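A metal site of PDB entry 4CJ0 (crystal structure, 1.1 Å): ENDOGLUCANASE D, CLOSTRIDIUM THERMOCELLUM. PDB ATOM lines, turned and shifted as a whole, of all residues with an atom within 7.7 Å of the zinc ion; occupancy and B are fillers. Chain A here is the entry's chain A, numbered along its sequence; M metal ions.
ND1 of His 150 is bound to the zinc ion. NE2 of His 173 is bound to the zinc ion, 2.1 Å away. SG of Cys 149 is bound to the zinc ion, at 2.3 Å. SG of Cys 131 binds the zinc ion (2.3 Å).
Residues that only touch the zinc ion: Gly 132 (3.9 Å). Within 4 Å of the zinc ion: Cys 131, Gly 132, Cys 149, His 150 and His 173.
A ring nitrogen (NE2) of His 150 sits at hydrogen-bond distance from the side-chain carboxylate (OE1) of Glu 261 (2.8 Å). The backbone NH of His 173 lies within hydrogen-bond range of the backbone carbonyl oxygen of Leu 129. The backbone NH (N) of Gly 132 lies close to the backbone carbonyl oxygen (O) of Cys 149 (3.0 Å). The side-chain sulfur (SG) of Cys 131 lies close to the guanidinium group (NH2) of Arg 265 (3.4 Å). The backbone carbonyl oxygen (O) of Gly 171 lies within hydrogen-bond range of the backbone NH (N) of Cys 131 (2.9 Å).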
ATOM      1  N   LEU A 129     -25.278  18.406   2.145  1.00  0.00           N
ATOM      2  CA  LEU A 129     -25.404  17.280   1.242  1.00  0.00           C
ATOM      3  C   LEU A 129     -26.132  17.641  -0.050  1.00  0.00           C
ATOM      4  O   LEU A 129     -26.226  16.779  -0.935  1.00  0.00           O
ATOM      5  CB  LEU A 129     -26.112  16.099   1.909  1.00  0.00           C
ATOM      6  CG  LEU A 129     -25.248  15.244   2.823  1.00  0.00           C
ATOM      7  CD1 LEU A 129     -26.139  14.311   3.625  1.00  0.00           C
ATOM      8  CD2 LEU A 129     -24.216  14.452   2.060  1.00  0.00           C
ATOM      9  N   ARG A 130     -26.645  18.856  -0.213  1.00  0.00           N
ATOM     10  CA  ARG A 130     -27.409  19.160  -1.410  1.00  0.00           C
ATOM     11  C   ARG A 130     -26.566  18.949  -2.693  1.00  0.00           C
ATOM     12  O   ARG A 130     -25.375  19.258  -2.749  1.00  0.00           O
ATOM     13  CB  ARG A 130     -27.938  20.582  -1.357  1.00  0.00           C
ATOM     14  CG  ARG A 130     -29.086  20.781  -0.394  1.00  0.00           C
ATOM     15  CD  ARG A 130     -29.586  22.213  -0.501  1.00  0.00           C
ATOM     16  NE  ARG A 130     -30.590  22.498   0.524  1.00  0.00           N
ATOM     17  CZ  ARG A 130     -31.305  23.619   0.526  1.00  0.00           C
ATOM     18  NH1 ARG A 130     -31.129  24.526  -0.406  1.00  0.00           N
ATOM     19  NH2 ARG A 130     -32.151  23.861   1.515  1.00  0.00           N
ATOM     20  N   CYS A 131     -27.269  18.470  -3.710  1.00  0.00           N
ATOM     21  CA  CYS A 131     -26.717  18.216  -5.027  1.00  0.00           C
ATOM     22  C   CYS A 131     -27.312  19.215  -6.033  1.00  0.00           C
ATOM     23  O   CYS A 131     -28.472  19.597  -5.882  1.00  0.00           O
ATOM     24  CB  CYS A 131     -27.055  16.798  -5.383  1.00  0.00           C
ATOM     25  SG  CYS A 131     -26.372  16.181  -6.961  1.00  0.00           S
ATOM     26  N   GLY A 132     -26.558  19.590  -7.055  1.00  0.00           N
ATOM     27  CA  GLY A 132     -27.061  20.451  -8.116  1.00  0.00           C
ATOM     28  C   GLY A 132     -26.895  21.922  -7.880  1.00  0.00           C
ATOM     29  O   GLY A 132     -27.301  22.692  -8.717  1.00  0.00           O
ATOM     30  N   THR A 133     -26.274  22.287  -6.786  1.00  0.00           N
ATOM     31  CA  THR A 133     -26.070  23.655  -6.389  1.00  0.00           C
ATOM     32  C   THR A 133     -24.733  23.763  -5.657  1.00  0.00           C
ATOM     33  O   THR A 133     -24.247  22.803  -5.126  1.00  0.00           O
ATOM     34  CB  THR A 133     -27.228  24.029  -5.351  1.00  0.00           C
ATOM     35  OG1 THR A 133     -27.063  25.271  -4.914  1.00  0.00           O
ATOM     36  CG2 THR A 133     -27.326  23.223  -4.178  1.00  0.00           C
ATOM     37  N   HIS A 146     -18.683  23.900  -1.551  1.00  0.00           N
ATOM     38  CA  HIS A 146     -18.350  23.367  -2.837  1.00  0.00           C
ATOM     39  C   HIS A 146     -19.164  24.049  -3.922  1.00  0.00           C
ATOM     40  O   HIS A 146     -20.217  24.601  -3.626  1.00  0.00           O
ATOM     41  CB  HIS A 146     -18.422  21.809  -2.910  1.00  0.00           C
ATOM     42  CG  HIS A 146     -19.802  21.236  -2.876  1.00  0.00           C
ATOM     43  ND1 HIS A 146     -20.750  21.408  -3.861  1.00  0.00           N
ATOM     44  CD2 HIS A 146     -20.362  20.404  -1.969  1.00  0.00           C
ATOM     45  CE1 HIS A 146     -21.826  20.718  -3.544  1.00  0.00           C
ATOM     46  NE2 HIS A 146     -21.633  20.078  -2.405  1.00  0.00           N
ATOM     47  N   GLY A 147     -18.701  23.983  -5.174  1.00  0.00           N
ATOM     48  CA  GLY A 147     -19.399  24.546  -6.286  1.00  0.00           C
ATOM     49  C   GLY A 147     -20.511  23.694  -6.784  1.00  0.00           C
ATOM     50  O   GLY A 147     -20.768  22.561  -6.314  1.00  0.00           O
ATOM     51  N   PRO A 148     -21.244  24.170  -7.805  1.00  0.00           N
ATOM     52  CA  PRO A 148     -22.422  23.413  -8.315  1.00  0.00           C
ATOM     53  C   PRO A 148     -21.977  22.044  -8.835  1.00  0.00           C
ATOM     54  O   PRO A 148     -21.016  21.953  -9.609  1.00  0.00           O
ATOM     55  CB  PRO A 148     -22.991  24.295  -9.392  1.00  0.00           C
ATOM     56  CG  PRO A 148     -22.459  25.677  -9.096  1.00  0.00           C
ATOM     57  CD  PRO A 148     -21.076  25.452  -8.528  1.00  0.00           C
ATOM     58  N   CYS A 149     -22.714  21.007  -8.505  1.00  0.00           N
ATOM     59  CA  CYS A 149     -22.355  19.647  -8.882  1.00  0.00           C
ATOM     60  C   CYS A 149     -23.515  18.956  -9.592  1.00  0.00           C
ATOM     61  O   CYS A 149     -24.690  19.204  -9.357  1.00  0.00           O
ATOM     62  CB  CYS A 149     -21.932  18.853  -7.665  1.00  0.00           C
ATOM     63  SG  CYS A 149     -23.228  18.689  -6.366  1.00  0.00           S
ATOM     64  N   HIS A 150     -23.149  17.997 -10.443  1.00  0.00           N
ATOM     65  CA  HIS A 150     -24.090  17.086 -11.050  1.00  0.00           C
ATOM     66  C   HIS A 150     -25.225  17.819 -11.701  1.00  0.00           C
ATOM     67  O   HIS A 150     -26.403  17.491 -11.626  1.00  0.00           O
ATOM     68  CB  HIS A 150     -24.594  16.044 -10.042  1.00  0.00           C
ATOM     69  CG  HIS A 150     -23.463  15.327  -9.409  1.00  0.00           C
ATOM     70  ND1 HIS A 150     -23.128  15.506  -8.079  1.00  0.00           N
ATOM     71  CD2 HIS A 150     -22.589  14.438  -9.917  1.00  0.00           C
ATOM     72  CE1 HIS A 150     -22.035  14.743  -7.823  1.00  0.00           C
ATOM     73  NE2 HIS A 150     -21.721  14.095  -8.929  1.00  0.00           N
ATOM     74  N   THR A 151     -24.869  18.863 -12.473  1.00  0.00           N
ATOM     75  CA  THR A 151     -25.791  19.727 -13.104  1.00  0.00           C
ATOM     76  C   THR A 151     -26.375  19.161 -14.409  1.00  0.00           C
ATOM     77  O   THR A 151     -27.281  19.738 -14.973  1.00  0.00           O
ATOM     78  CB  THR A 151     -25.195  21.113 -13.323  1.00  0.00           C
ATOM     79  OG1 THR A 151     -24.111  20.968 -14.223  1.00  0.00           O
ATOM     80  CG2 THR A 151     -24.758  21.772 -12.064  1.00  0.00           C
ATOM     81  N   ASP A 153     -27.645  15.959 -14.516  1.00  0.00           N
ATOM     82  CA  ASP A 153     -28.471  14.836 -14.176  1.00  0.00           C
ATOM     83  C   ASP A 153     -29.783  14.938 -14.965  1.00  0.00           C
ATOM     84  O   ASP A 153     -30.392  16.001 -14.926  1.00  0.00           O
ATOM     85  CB  ASP A 153     -28.815  14.855 -12.688  1.00  0.00           C
ATOM     86  CG  ASP A 153     -27.705  14.462 -11.754  1.00  0.00           C
ATOM     87  OD1 ASP A 153     -26.630  14.034 -12.228  1.00  0.00           O
ATOM     88  OD2 ASP A 153     -27.973  14.506 -10.527  1.00  0.00           O
ATOM     89  N   LYS A 170     -30.917  18.341  -8.195  1.00  0.00           N
ATOM     90  CA  LYS A 170     -31.356  18.680  -6.821  1.00  0.00           C
ATOM     91  C   LYS A 170     -31.364  17.426  -5.954  1.00  0.00           C
ATOM     92  O   LYS A 170     -30.674  16.440  -6.263  1.00  0.00           O
ATOM     93  CB  LYS A 170     -32.676  19.490  -6.773  1.00  0.00           C
ATOM     94  CG  LYS A 170     -32.680  20.673  -7.729  1.00  0.00           C
ATOM     95  CD  LYS A 170     -33.943  21.473  -7.653  1.00  0.00           C
ATOM     96  CE  LYS A 170     -33.975  22.361  -6.484  1.00  0.00           C
ATOM     97  NZ  LYS A 170     -35.106  23.300  -6.596  1.00  0.00           N
ATOM     98  N   GLY A 171     -32.064  17.458  -4.829  1.00  0.00           N
ATOM     99  CA  GLY A 171     -31.941  16.362  -3.878  1.00  0.00           C
ATOM    100  C   GLY A 171     -30.651  16.403  -3.084  1.00  0.00           C
ATOM    101  O   GLY A 171     -29.819  17.286  -3.235  1.00  0.00           O
ATOM    102  N   TRP A 172     -30.517  15.381  -2.229  1.00  0.00           N
ATOM    103  CA  TRP A 172     -29.361  15.191  -1.391  1.00  0.00           C
ATOM    104  C   TRP A 172     -28.484  14.084  -1.922  1.00  0.00           C
ATOM    105  O   TRP A 172     -28.957  12.978  -2.236  1.00  0.00           O
ATOM    106  CB  TRP A 172     -29.748  14.854   0.038  1.00  0.00           C
ATOM    107  CG  TRP A 172     -30.590  15.826   0.775  1.00  0.00           C
ATOM    108  CD1 TRP A 172     -30.399  17.178   0.949  1.00  0.00           C
ATOM    109  CD2 TRP A 172     -31.829  15.534   1.457  1.00  0.00           C
ATOM    110  NE1 TRP A 172     -31.429  17.733   1.642  1.00  0.00           N
ATOM    111  CE2 TRP A 172     -32.329  16.748   1.978  1.00  0.00           C
ATOM    112  CE3 TRP A 172     -32.559  14.335   1.663  1.00  0.00           C
ATOM    113  CZ2 TRP A 172     -33.499  16.795   2.720  1.00  0.00           C
ATOM    114  CZ3 TRP A 172     -33.699  14.387   2.441  1.00  0.00           C
ATOM    115  CH2 TRP A 172     -34.166  15.631   2.932  1.00  0.00           C
ATOM    116  N   HIS A 173     -27.177  14.307  -1.926  1.00  0.00           N
ATOM    117  CA  HIS A 173     -26.227  13.217  -1.998  1.00  0.00           C
ATOM    118  C   HIS A 173     -26.559  12.237  -0.867  1.00  0.00           C
ATOM    119  O   HIS A 173     -26.799  12.637   0.261  1.00  0.00           O
ATOM    120  CB  HIS A 173     -24.802  13.768  -1.822  1.00  0.00           C
ATOM    121  CG  HIS A 173     -24.372  14.715  -2.881  1.00  0.00           C
ATOM    122  ND1 HIS A 173     -23.675  15.865  -2.595  1.00  0.00           N
ATOM    123  CD2 HIS A 173     -24.462  14.663  -4.208  1.00  0.00           C
ATOM    124  CE1 HIS A 173     -23.390  16.497  -3.732  1.00  0.00           C
ATOM    125  NE2 HIS A 173     -23.852  15.770  -4.730  1.00  0.00           N
ATOM    126  N   TYR A 178     -22.056  10.372  -3.961  1.00  0.00           N
ATOM    127  CA  TYR A 178     -22.884  11.432  -4.454  1.00  0.00           C
ATOM    128  C   TYR A 178     -24.140  10.996  -5.148  1.00  0.00           C
ATOM    129  O   TYR A 178     -24.946  11.811  -5.616  1.00  0.00           O
ATOM    130  CB  TYR A 178     -22.085  12.365  -5.375  1.00  0.00           C
ATOM    131  CG  TYR A 178     -20.849  12.928  -4.741  1.00  0.00           C
ATOM    132  CD1 TYR A 178     -20.926  13.597  -3.541  1.00  0.00           C
ATOM    133  CD2 TYR A 178     -19.586  12.827  -5.324  1.00  0.00           C
ATOM    134  CE1 TYR A 178     -19.832  14.162  -2.940  1.00  0.00           C
ATOM    135  CE2 TYR A 178     -18.439  13.398  -4.714  1.00  0.00           C
ATOM    136  CZ  TYR A 178     -18.581  14.060  -3.505  1.00  0.00           C
ATOM    137  OH  TYR A 178     -17.501  14.657  -2.889  1.00  0.00           O
ATOM    138  N   ASN A 179     -24.353   9.686  -5.296  1.00  0.00           N
ATOM    139  CA  ASN A 179     -25.521   9.181  -6.021  1.00  0.00           C
ATOM    140  C   ASN A 179     -26.785   9.375  -5.170  1.00  0.00           C
ATOM    141  O   ASN A 179     -26.703   9.684  -3.968  1.00  0.00           O
ATOM    142  CB  ASN A 179     -25.288   7.733  -6.426  1.00  0.00           C
ATOM    143  CG  ASN A 179     -23.999   7.641  -7.241  1.00  0.00           C
ATOM    144  OD1 ASN A 179     -23.905   8.118  -8.368  1.00  0.00           O
ATOM    145  ND2 ASN A 179     -22.951   7.066  -6.623  1.00  0.00           N
ATOM    146  N   LYS A 180     -27.947   9.218  -5.802  1.00  0.00           N
ATOM    147  CA  LYS A 180     -29.238   9.589  -5.209  1.00  0.00           C
ATOM    148  C   LYS A 180     -30.180   8.417  -5.404  1.00  0.00           C
ATOM    149  O   LYS A 180     -30.412   7.978  -6.523  1.00  0.00           O
ATOM    150  CB  LYS A 180     -29.745  10.912  -5.855  1.00  0.00           C
ATOM    151  CG  LYS A 180     -28.770  12.029  -5.728  1.00  0.00           C
ATOM    152  CD  LYS A 180     -29.237  13.399  -6.224  1.00  0.00           C
ATOM    153  CE  LYS A 180     -29.662  13.371  -7.682  1.00  0.00           C
ATOM    154  NZ  LYS A 180     -29.730  14.761  -8.245  1.00  0.00           N
ATOM    155  N   PRO A 258     -17.572  17.096  -5.417  1.00  0.00           N
ATOM    156  CA  PRO A 258     -18.641  16.675  -6.367  1.00  0.00           C
ATOM    157  C   PRO A 258     -18.670  17.463  -7.677  1.00  0.00           C
ATOM    158  O   PRO A 258     -19.054  16.925  -8.706  1.00  0.00           O
ATOM    159  CB  PRO A 258     -19.914  16.793  -5.544  1.00  0.00           C
ATOM    160  CG  PRO A 258     -19.575  17.871  -4.503  1.00  0.00           C
ATOM    161  CD  PRO A 258     -18.119  17.600  -4.171  1.00  0.00           C
ATOM    162  N   GLU A 259     -18.272  18.740  -7.588  1.00  0.00           N
ATOM    163  CA  GLU A 259     -18.228  19.567  -8.786  1.00  0.00           C
ATOM    164  C   GLU A 259     -17.117  19.130  -9.741  1.00  0.00           C
ATOM    165  O   GLU A 259     -17.087  19.598 -10.891  1.00  0.00           O
ATOM    166  CB  GLU A 259     -18.014  21.095  -8.447  1.00  0.00           C
ATOM    167  CG  GLU A 259     -16.713  21.455  -7.793  1.00  0.00           C
ATOM    168  CD  GLU A 259     -16.792  21.381  -6.292  1.00  0.00           C
ATOM    169  OE1 GLU A 259     -17.279  20.423  -5.730  1.00  0.00           O
ATOM    170  OE2 GLU A 259     -16.300  22.393  -5.706  1.00  0.00           O
ATOM    171  N   GLU A 261     -16.716  15.850 -10.475  1.00  0.00           N
ATOM    172  CA  GLU A 261     -17.153  14.547 -10.978  1.00  0.00           C
ATOM    173  C   GLU A 261     -17.970  14.752 -12.234  1.00  0.00           C
ATOM    174  O   GLU A 261     -19.178  15.094 -12.130  1.00  0.00           O
ATOM    175  CB  GLU A 261     -17.977  13.797  -9.910  1.00  0.00           C
ATOM    176  CG  GLU A 261     -18.295  12.405 -10.392  1.00  0.00           C
ATOM    177  CD  GLU A 261     -18.973  11.536  -9.346  1.00  0.00           C
ATOM    178  OE1 GLU A 261     -20.002  11.928  -8.810  1.00  0.00           O
ATOM    179  OE2 GLU A 261     -18.387  10.420  -9.099  1.00  0.00           O
ATOM    180  N   ARG A 265     -24.358  10.650 -15.422  1.00  0.00           N
ATOM    181  CA  ARG A 265     -25.227  10.027 -14.480  1.00  0.00           C
ATOM    182  C   ARG A 265     -26.518   9.619 -15.163  1.00  0.00           C
ATOM    183  O   ARG A 265     -26.997  10.323 -16.087  1.00  0.00           O
ATOM    184  CB  ARG A 265     -25.525  10.911 -13.271  1.00  0.00           C
ATOM    185  CG  ARG A 265     -24.218  11.406 -12.609  1.00  0.00           C
ATOM    186  CD  ARG A 265     -24.222  11.375 -11.107  1.00  0.00           C
ATOM    187  NE  ARG A 265     -25.222  12.275 -10.555  1.00  0.00           N
ATOM    188  CZ  ARG A 265     -25.334  12.499  -9.236  1.00  0.00           C
ATOM    189  NH1 ARG A 265     -24.516  11.902  -8.370  1.00  0.00           N
ATOM    190  NH2 ARG A 265     -26.281  13.287  -8.802  1.00  0.00           N
HETATM  191 ZN    ZN M   1     -24.108  16.567  -6.654  1.00  0.00          ZN
